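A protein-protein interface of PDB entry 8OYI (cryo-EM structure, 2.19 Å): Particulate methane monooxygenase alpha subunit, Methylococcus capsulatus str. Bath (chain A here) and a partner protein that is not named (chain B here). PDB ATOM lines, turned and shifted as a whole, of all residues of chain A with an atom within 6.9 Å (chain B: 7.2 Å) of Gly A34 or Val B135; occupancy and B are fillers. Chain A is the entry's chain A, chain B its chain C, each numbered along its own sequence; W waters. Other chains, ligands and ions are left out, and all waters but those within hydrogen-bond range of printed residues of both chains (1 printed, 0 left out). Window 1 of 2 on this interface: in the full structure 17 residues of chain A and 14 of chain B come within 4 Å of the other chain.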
ATOM      1  N   HIS A  33      -0.294   3.719 -22.619  1.00  0.00           N
ATOM      2  CA  HIS A  33       0.097   3.805 -21.214  1.00  0.00           C
ATOM      3  C   HIS A  33      -0.687   2.648 -20.613  1.00  0.00           C
ATOM      4  O   HIS A  33      -0.379   2.243 -19.482  1.00  0.00           O
ATOM      5  CB  HIS A  33      -0.301   5.138 -20.540  1.00  0.00           C
ATOM      6  CG  HIS A  33       0.786   6.166 -20.444  1.00  0.00           C
ATOM      7  ND1 HIS A  33       1.685   6.308 -21.466  1.00  0.00           N
ATOM      8  CD2 HIS A  33       1.117   7.107 -19.509  1.00  0.00           C
ATOM      9  CE1 HIS A  33       2.556   7.247 -21.152  1.00  0.00           C
ATOM     10  NE2 HIS A  33       2.207   7.785 -19.998  1.00  0.00           N
ATOM     11  N   GLY A  34      -1.660   2.141 -21.387  1.00  0.00           N
ATOM     12  CA  GLY A  34      -2.490   1.005 -20.949  1.00  0.00           C
ATOM     13  C   GLY A  34      -1.934  -0.326 -21.418  1.00  0.00           C
ATOM     14  O   GLY A  34      -2.624  -1.342 -21.231  1.00  0.00           O
ATOM     15  N   GLU A  35      -0.794  -0.340 -22.108  1.00  0.00           N
ATOM     16  CA  GLU A  35      -0.183  -1.657 -22.448  1.00  0.00           C
ATOM     17  C   GLU A  35       0.898  -1.947 -21.394  1.00  0.00           C
ATOM     18  O   GLU A  35       0.873  -1.253 -20.348  1.00  0.00           O
ATOM     19  CB  GLU A  35       0.231  -1.724 -23.927  1.00  0.00           C
ATOM     20  CG  GLU A  35       1.669  -1.355 -24.216  1.00  0.00           C
ATOM     21  CD  GLU A  35       2.004   0.065 -23.809  1.00  0.00           C
ATOM     22  OE1 GLU A  35       1.586   0.993 -24.518  1.00  0.00           O
ATOM     23  OE2 GLU A  35       2.655   0.224 -22.765  1.00  0.00           O
ATOM     24  N   LYS A  36       1.777  -2.930 -21.621  1.00  0.00           N
ATOM     25  CA  LYS A  36       2.773  -3.354 -20.589  1.00  0.00           C
ATOM     26  C   LYS A  36       2.026  -4.079 -19.463  1.00  0.00           C
ATOM     27  O   LYS A  36       2.702  -4.553 -18.546  1.00  0.00           O
ATOM     28  CB  LYS A  36       3.573  -2.180 -20.010  1.00  0.00           C
ATOM     29  CG  LYS A  36       4.694  -1.642 -20.881  1.00  0.00           C
ATOM     30  CD  LYS A  36       4.973  -0.175 -20.638  1.00  0.00           C
ATOM     31  CE  LYS A  36       6.426   0.116 -20.333  1.00  0.00           C
ATOM     32  NZ  LYS A  36       6.636   0.371 -18.887  1.00  0.00           N
ATOM     33  N   SER A  37       0.691  -4.138 -19.523  1.00  0.00           N
ATOM     34  CA  SER A  37      -0.138  -4.832 -18.508  1.00  0.00           C
ATOM     35  C   SER A  37      -0.932  -5.936 -19.203  1.00  0.00           C
ATOM     36  O   SER A  37      -1.239  -6.933 -18.538  1.00  0.00           O
ATOM     37  CB  SER A  37      -1.052  -3.869 -17.807  1.00  0.00           C
ATOM     38  OG  SER A  37      -0.305  -2.860 -17.150  1.00  0.00           O
ATOM     39  N   GLN A  38      -1.242  -5.768 -20.494  1.00  0.00           N
ATOM     40  CA  GLN A  38      -1.909  -6.835 -21.217  1.00  0.00           C
ATOM     41  C   GLN A  38      -0.967  -8.015 -21.422  1.00  0.00           C
ATOM     42  O   GLN A  38       0.259  -7.894 -21.335  1.00  0.00           O
ATOM     43  CB  GLN A  38      -2.423  -6.328 -22.564  1.00  0.00           C
ATOM     44  CG  GLN A  38      -2.877  -4.884 -22.547  1.00  0.00           C
ATOM     45  CD  GLN A  38      -3.398  -4.428 -23.892  1.00  0.00           C
ATOM     46  OE1 GLN A  38      -2.662  -3.857 -24.693  1.00  0.00           O
ATOM     47  NE2 GLN A  38      -4.678  -4.675 -24.146  1.00  0.00           N
ATOM     48  N   ARG A  43      -0.619  -9.265 -26.962  1.00  0.00           N
ATOM     49  CA  ARG A  43      -0.040  -8.110 -27.636  1.00  0.00           C
ATOM     50  C   ARG A  43       0.755  -8.527 -28.863  1.00  0.00           C
ATOM     51  O   ARG A  43       0.805  -7.791 -29.854  1.00  0.00           O
ATOM     52  CB  ARG A  43       0.845  -7.323 -26.672  1.00  0.00           C
ATOM     53  CG  ARG A  43       0.080  -6.424 -25.721  1.00  0.00           C
ATOM     54  CD  ARG A  43       1.024  -5.565 -24.907  1.00  0.00           C
ATOM     55  NE  ARG A  43       1.578  -6.297 -23.777  1.00  0.00           N
ATOM     56  CZ  ARG A  43       2.839  -6.217 -23.376  1.00  0.00           C
ATOM     57  NH1 ARG A  43       3.707  -5.429 -23.988  1.00  0.00           N
ATOM     58  NH2 ARG A  43       3.239  -6.944 -22.338  1.00  0.00           N
ATOM     59  N   GLY A  92      -5.229   6.434 -28.252  1.00  0.00           N
ATOM     60  CA  GLY A  92      -4.883   6.285 -26.853  1.00  0.00           C
ATOM     61  C   GLY A  92      -4.269   7.550 -26.296  1.00  0.00           C
ATOM     62  O   GLY A  92      -3.171   7.943 -26.700  1.00  0.00           O
ATOM     63  N   MET A  93      -4.963   8.197 -25.366  1.00  0.00           N
ATOM     64  CA  MET A  93      -4.553   9.507 -24.886  1.00  0.00           C
ATOM     65  C   MET A  93      -5.266   9.790 -23.574  1.00  0.00           C
ATOM     66  O   MET A  93      -6.330   9.220 -23.303  1.00  0.00           O
ATOM     67  CB  MET A  93      -4.865  10.585 -25.927  1.00  0.00           C
ATOM     68  CG  MET A  93      -6.278  11.109 -25.876  1.00  0.00           C
ATOM     69  SD  MET A  93      -6.751  11.943 -27.399  1.00  0.00           S
ATOM     70  CE  MET A  93      -5.140  12.417 -28.002  1.00  0.00           C
ATOM     71  N   HIS A 139      -1.170   7.223 -28.456  1.00  0.00           N
ATOM     72  CA  HIS A 139      -1.174   5.892 -29.039  1.00  0.00           C
ATOM     73  C   HIS A 139      -2.237   5.813 -30.123  1.00  0.00           C
ATOM     74  O   HIS A 139      -3.300   6.431 -30.017  1.00  0.00           O
ATOM     75  CB  HIS A 139      -1.456   4.813 -27.986  1.00  0.00           C
ATOM     76  CG  HIS A 139      -0.413   4.707 -26.922  1.00  0.00           C
ATOM     77  ND1 HIS A 139       0.495   3.673 -26.868  1.00  0.00           N
ATOM     78  CD2 HIS A 139      -0.143   5.501 -25.858  1.00  0.00           C
ATOM     79  CE1 HIS A 139       1.283   3.835 -25.822  1.00  0.00           C
ATOM     80  NE2 HIS A 139       0.918   4.938 -25.193  1.00  0.00           N
ATOM     81  N   MET A 141      -4.725   3.106 -31.515  1.00  0.00           N
ATOM     82  CA  MET A 141      -5.251   1.864 -30.986  1.00  0.00           C
ATOM     83  C   MET A 141      -6.454   1.389 -31.789  1.00  0.00           C
ATOM     84  O   MET A 141      -7.134   2.161 -32.467  1.00  0.00           O
ATOM     85  CB  MET A 141      -5.624   2.030 -29.515  1.00  0.00           C
ATOM     86  CG  MET A 141      -6.470   3.250 -29.240  1.00  0.00           C
ATOM     87  SD  MET A 141      -6.936   3.394 -27.508  1.00  0.00           S
ATOM     88  CE  MET A 141      -7.383   1.702 -27.141  1.00  0.00           C
ATOM     89  N   ASN A 143      -9.912  -0.770 -31.041  1.00  0.00           N
ATOM     90  CA  ASN A 143     -10.833  -1.397 -30.108  1.00  0.00           C
ATOM     91  C   ASN A 143     -11.666  -2.416 -30.873  1.00  0.00           C
ATOM     92  O   ASN A 143     -12.251  -2.090 -31.910  1.00  0.00           O
ATOM     93  CB  ASN A 143     -11.729  -0.359 -29.434  1.00  0.00           C
ATOM     94  CG  ASN A 143     -10.979   0.503 -28.440  1.00  0.00           C
ATOM     95  OD1 ASN A 143     -10.809   1.703 -28.650  1.00  0.00           O
ATOM     96  ND2 ASN A 143     -10.535  -0.103 -27.349  1.00  0.00           N
ATOM     97  N   PRO A 149      -9.170  -3.402 -25.912  1.00  0.00           N
ATOM     98  CA  PRO A 149      -8.258  -2.487 -26.614  1.00  0.00           C
ATOM     99  C   PRO A 149      -6.983  -3.140 -27.125  1.00  0.00           C
ATOM    100  O   PRO A 149      -6.345  -3.922 -26.416  1.00  0.00           O
ATOM    101  CB  PRO A 149      -7.945  -1.436 -25.546  1.00  0.00           C
ATOM    102  CG  PRO A 149      -8.051  -2.177 -24.257  1.00  0.00           C
ATOM    103  CD  PRO A 149      -9.041  -3.303 -24.448  1.00  0.00           C
ATOM    104  N   ILE A 151      -3.577  -1.731 -28.242  1.00  0.00           N
ATOM    105  CA  ILE A 151      -2.850  -0.471 -28.241  1.00  0.00           C
ATOM    106  C   ILE A 151      -1.583  -0.599 -29.073  1.00  0.00           C
ATOM    107  O   ILE A 151      -0.762  -1.500 -28.854  1.00  0.00           O
ATOM    108  CB  ILE A 151      -2.530  -0.032 -26.805  1.00  0.00           C
ATOM    109  CG1 ILE A 151      -3.817   0.090 -25.988  1.00  0.00           C
ATOM    110  CG2 ILE A 151      -1.772   1.278 -26.800  1.00  0.00           C
ATOM    111  CD1 ILE A 151      -3.826  -0.749 -24.737  1.00  0.00           C
ATOM    112  N   LEU B  49      -0.685   7.156 -14.498  1.00  0.00           N
ATOM    113  CA  LEU B  49      -1.202   6.568 -15.729  1.00  0.00           C
ATOM    114  C   LEU B  49      -0.592   5.191 -15.990  1.00  0.00           C
ATOM    115  O   LEU B  49      -1.289   4.259 -16.400  1.00  0.00           O
ATOM    116  CB  LEU B  49      -0.946   7.506 -16.910  1.00  0.00           C
ATOM    117  CG  LEU B  49      -2.001   8.583 -17.164  1.00  0.00           C
ATOM    118  CD1 LEU B  49      -1.983   9.012 -18.621  1.00  0.00           C
ATOM    119  CD2 LEU B  49      -3.382   8.086 -16.774  1.00  0.00           C
ATOM    120  N   ASP B  50       0.713   5.053 -15.763  1.00  0.00           N
ATOM    121  CA  ASP B  50       1.406   3.793 -16.005  1.00  0.00           C
ATOM    122  C   ASP B  50       1.583   3.051 -14.687  1.00  0.00           C
ATOM    123  O   ASP B  50       2.337   3.495 -13.815  1.00  0.00           O
ATOM    124  CB  ASP B  50       2.755   4.049 -16.672  1.00  0.00           C
ATOM    125  CG  ASP B  50       3.524   2.770 -16.949  1.00  0.00           C
ATOM    126  OD1 ASP B  50       2.909   1.685 -16.964  1.00  0.00           O
ATOM    127  OD2 ASP B  50       4.753   2.854 -17.167  1.00  0.00           O
ATOM    128  N   TRP B 130     -12.906   8.422 -15.135  1.00  0.00           N
ATOM    129  CA  TRP B 130     -11.526   7.869 -15.205  1.00  0.00           C
ATOM    130  C   TRP B 130     -11.479   6.720 -16.217  1.00  0.00           C
ATOM    131  O   TRP B 130     -10.707   6.822 -17.189  1.00  0.00           O
ATOM    132  CB  TRP B 130     -11.057   7.415 -13.816  1.00  0.00           C
ATOM    133  CG  TRP B 130      -9.796   6.606 -13.836  1.00  0.00           C
ATOM    134  CD1 TRP B 130      -9.641   5.330 -14.294  1.00  0.00           C
ATOM    135  CD2 TRP B 130      -8.497   7.020 -13.374  1.00  0.00           C
ATOM    136  NE1 TRP B 130      -8.343   4.923 -14.151  1.00  0.00           N
ATOM    137  CE2 TRP B 130      -7.617   5.939 -13.591  1.00  0.00           C
ATOM    138  CE3 TRP B 130      -7.994   8.193 -12.803  1.00  0.00           C
ATOM    139  CZ2 TRP B 130      -6.266   6.000 -13.252  1.00  0.00           C
ATOM    140  CZ3 TRP B 130      -6.659   8.252 -12.467  1.00  0.00           C
ATOM    141  CH2 TRP B 130      -5.808   7.170 -12.691  1.00  0.00           C
ATOM    142  N   HIS B 131     -12.266   5.665 -15.988  1.00  0.00           N
ATOM    143  CA  HIS B 131     -12.249   4.481 -16.889  1.00  0.00           C
ATOM    144  C   HIS B 131     -12.688   4.875 -18.303  1.00  0.00           C
ATOM    145  O   HIS B 131     -12.078   4.372 -19.267  1.00  0.00           O
ATOM    146  CB  HIS B 131     -13.123   3.368 -16.300  1.00  0.00           C
ATOM    147  CG  HIS B 131     -12.605   2.853 -15.001  1.00  0.00           C
ATOM    148  ND1 HIS B 131     -11.285   2.988 -14.634  1.00  0.00           N
ATOM    149  CD2 HIS B 131     -13.212   2.216 -13.978  1.00  0.00           C
ATOM    150  CE1 HIS B 131     -11.110   2.454 -13.443  1.00  0.00           C
ATOM    151  NE2 HIS B 131     -12.255   1.966 -13.029  1.00  0.00           N
ATOM    152  N   GLN B 132     -13.700   5.737 -18.419  1.00  0.00           N
ATOM    153  CA  GLN B 132     -14.233   6.131 -19.750  1.00  0.00           C
ATOM    154  C   GLN B 132     -13.176   6.933 -20.518  1.00  0.00           C
ATOM    155  O   GLN B 132     -13.384   7.162 -21.727  1.00  0.00           O
ATOM    156  CB  GLN B 132     -15.503   6.965 -19.585  1.00  0.00           C
ATOM    157  CG  GLN B 132     -16.653   6.198 -18.949  1.00  0.00           C
ATOM    158  CD  GLN B 132     -17.265   5.206 -19.907  1.00  0.00           C
ATOM    159  OE1 GLN B 132     -18.210   5.514 -20.629  1.00  0.00           O
ATOM    160  NE2 GLN B 132     -16.720   4.001 -19.922  1.00  0.00           N
ATOM    161  N   THR B 133     -12.091   7.338 -19.852  1.00  0.00           N
ATOM    162  CA  THR B 133     -11.091   8.212 -20.524  1.00  0.00           C
ATOM    163  C   THR B 133      -9.751   7.491 -20.704  1.00  0.00           C
ATOM    164  O   THR B 133      -9.053   7.816 -21.683  1.00  0.00           O
ATOM    165  CB  THR B 133     -10.900   9.528 -19.759  1.00  0.00           C
ATOM    166  OG1 THR B 133     -10.366   9.225 -18.469  1.00  0.00           O
ATOM    167  CG2 THR B 133     -12.184  10.312 -19.612  1.00  0.00           C
ATOM    168  N   ILE B 134      -9.389   6.568 -19.805  1.00  0.00           N
ATOM    169  CA  ILE B 134      -8.067   5.966 -19.931  1.00  0.00           C
ATOM    170  C   ILE B 134      -8.230   4.464 -20.114  1.00  0.00           C
ATOM    171  O   ILE B 134      -9.320   3.919 -19.916  1.00  0.00           O
ATOM    172  CB  ILE B 134      -7.157   6.294 -18.729  1.00  0.00           C
ATOM    173  CG1 ILE B 134      -7.744   5.773 -17.413  1.00  0.00           C
ATOM    174  CG2 ILE B 134      -6.904   7.792 -18.643  1.00  0.00           C
ATOM    175  CD1 ILE B 134      -7.220   4.417 -16.993  1.00  0.00           C
ATOM    176  N   VAL B 135      -7.153   3.787 -20.493  1.00  0.00           N
ATOM    177  CA  VAL B 135      -7.121   2.333 -20.570  1.00  0.00           C
ATOM    178  C   VAL B 135      -6.666   1.843 -19.207  1.00  0.00           C
ATOM    179  O   VAL B 135      -5.523   2.093 -18.801  1.00  0.00           O
ATOM    180  CB  VAL B 135      -6.193   1.825 -21.680  1.00  0.00           C
ATOM    181  CG1 VAL B 135      -6.071   0.313 -21.611  1.00  0.00           C
ATOM    182  CG2 VAL B 135      -6.711   2.251 -23.039  1.00  0.00           C
ATOM    183  N   ARG B 136      -7.553   1.160 -18.489  1.00  0.00           N
ATOM    184  CA  ARG B 136      -7.225   0.734 -17.137  1.00  0.00           C
ATOM    185  C   ARG B 136      -6.083  -0.273 -17.168  1.00  0.00           C
ATOM    186  O   ARG B 136      -6.087  -1.225 -17.951  1.00  0.00           O
ATOM    187  CB  ARG B 136      -8.464   0.162 -16.444  1.00  0.00           C
ATOM    188  CG  ARG B 136      -9.026  -1.107 -17.048  1.00  0.00           C
ATOM    189  CD  ARG B 136      -9.995  -1.779 -16.090  1.00  0.00           C
ATOM    190  NE  ARG B 136     -11.324  -1.178 -16.162  1.00  0.00           N
ATOM    191  CZ  ARG B 136     -12.065  -0.866 -15.109  1.00  0.00           C
ATOM    192  NH1 ARG B 136     -11.635  -1.075 -13.874  1.00  0.00           N
ATOM    193  NH2 ARG B 136     -13.268  -0.333 -15.299  1.00  0.00           N
ATOM    194  N   ASP B 137      -5.085  -0.035 -16.319  1.00  0.00           N
ATOM    195  CA  ASP B 137      -3.827  -0.757 -16.363  1.00  0.00           C
ATOM    196  C   ASP B 137      -3.686  -1.806 -15.272  1.00  0.00           C
ATOM    197  O   ASP B 137      -2.750  -2.609 -15.327  1.00  0.00           O
ATOM    198  CB  ASP B 137      -2.653   0.228 -16.262  1.00  0.00           C
ATOM    199  CG  ASP B 137      -1.608   0.005 -17.327  1.00  0.00           C
ATOM    200  OD1 ASP B 137      -1.931  -0.643 -18.342  1.00  0.00           O
ATOM    201  OD2 ASP B 137      -0.466   0.473 -17.148  1.00  0.00           O
ATOM    202  N   THR B 138      -4.579  -1.822 -14.289  1.00  0.00           N
ATOM    203  CA  THR B 138      -4.430  -2.687 -13.129  1.00  0.00           C
ATOM    204  C   THR B 138      -5.737  -2.663 -12.353  1.00  0.00           C
ATOM    205  O   THR B 138      -6.663  -1.913 -12.680  1.00  0.00           O
ATOM    206  CB  THR B 138      -3.269  -2.244 -12.232  1.00  0.00           C
ATOM    207  OG1 THR B 138      -3.226  -3.063 -11.059  1.00  0.00           O
ATOM    208  CG2 THR B 138      -3.446  -0.792 -11.824  1.00  0.00           C
ATOM    209  N   GLU B 209     -15.535  -1.060 -21.590  1.00  0.00           N
ATOM    210  CA  GLU B 209     -15.767  -0.220 -20.388  1.00  0.00           C
ATOM    211  C   GLU B 209     -17.213   0.274 -20.421  1.00  0.00           C
ATOM    212  O   GLU B 209     -17.424   1.434 -20.807  1.00  0.00           O
ATOM    213  CB  GLU B 209     -14.779   0.947 -20.326  1.00  0.00           C
ATOM    214  CG  GLU B 209     -13.356   0.520 -20.031  1.00  0.00           C
ATOM    215  CD  GLU B 209     -13.086   0.187 -18.574  1.00  0.00           C
ATOM    216  OE1 GLU B 209     -13.908  -0.530 -17.972  1.00  0.00           O
ATOM    217  OE2 GLU B 209     -12.053   0.644 -18.049  1.00  0.00           O
HETATM  218  O   HOH W   1      -4.454  -2.972 -20.196  1.00  0.00           O
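O of Trp B130 lies within hydrogen-bond range of OG1 of Thr B133 (2.7 Å).
His A33 touches Leu B49.
Val B135 touches Gly A34 (CG1 to CA, 3.7 Å).
Glu A35 touches Asp B137.
Ile A151 touches Val B135.
Of the 14 printed residues of chain A, 7 touch a printed residue of chain B.
Hydrophobic or aromatic side chains of chain B that line the printed part of chain A: Leu B49 and Val B135.
Among the printed residues, 9 pairs touch across the chains.
Among the printed residues, Asp or Glu carboxylates within 4 Å of a Lys or Arg side-chain nitrogen of the other chain: Lys A36 with Asp B50 (3.6 Å).
Gly A34 touches two residues of chain B.
Of the printed residues of chain A, Val B135 touches Gly A34 (3.7 Å) and Ile A151 (3.99 Å).
Of the printed residues of chain B, His A33 touches Leu B49 (3.3 Å) and Asp B137 (2.9 Å).
Of the printed residues of chain B, Ser A37 touches Asp B137 (3.0 Å).
Of the printed residues of chain B, Lys A36 touches Asp B50 (3.6 Å).
Glu B209 touches none of the printed residues of chain A.
The nearest printed residue of chain B that does not touch Met A93 is Ile B134 (4.9 Å).
Water W1 lies within hydrogen-bond range of the backbone carbonyl oxygen of Gly A34 (2.7 Å) and the backbone carbonyl oxygen of Arg B136 (3.3 Å).
OD2 of Asp B137 sits close to O of His A33.
The side-chain hydroxyl (OG) of Ser A37 sits at hydrogen-bond distance from the side-chain carboxylate (OD1) of Asp B137, at 3.0 Å.
The backbone carbonyl oxygen of Gly A34 lies close to the side-chain carboxylate of Asp B137 (3.1 Å).
The backbone carbonyl oxygen (O) of Met A93 sits close to the backbone carbonyl oxygen (O) of Thr B133 (3.5 Å).
The side-chain amino group (NZ) of Lys A36 is in salt-bridge range of the side-chain carboxylate (OD2) of Asp B50 (3.6 Å).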
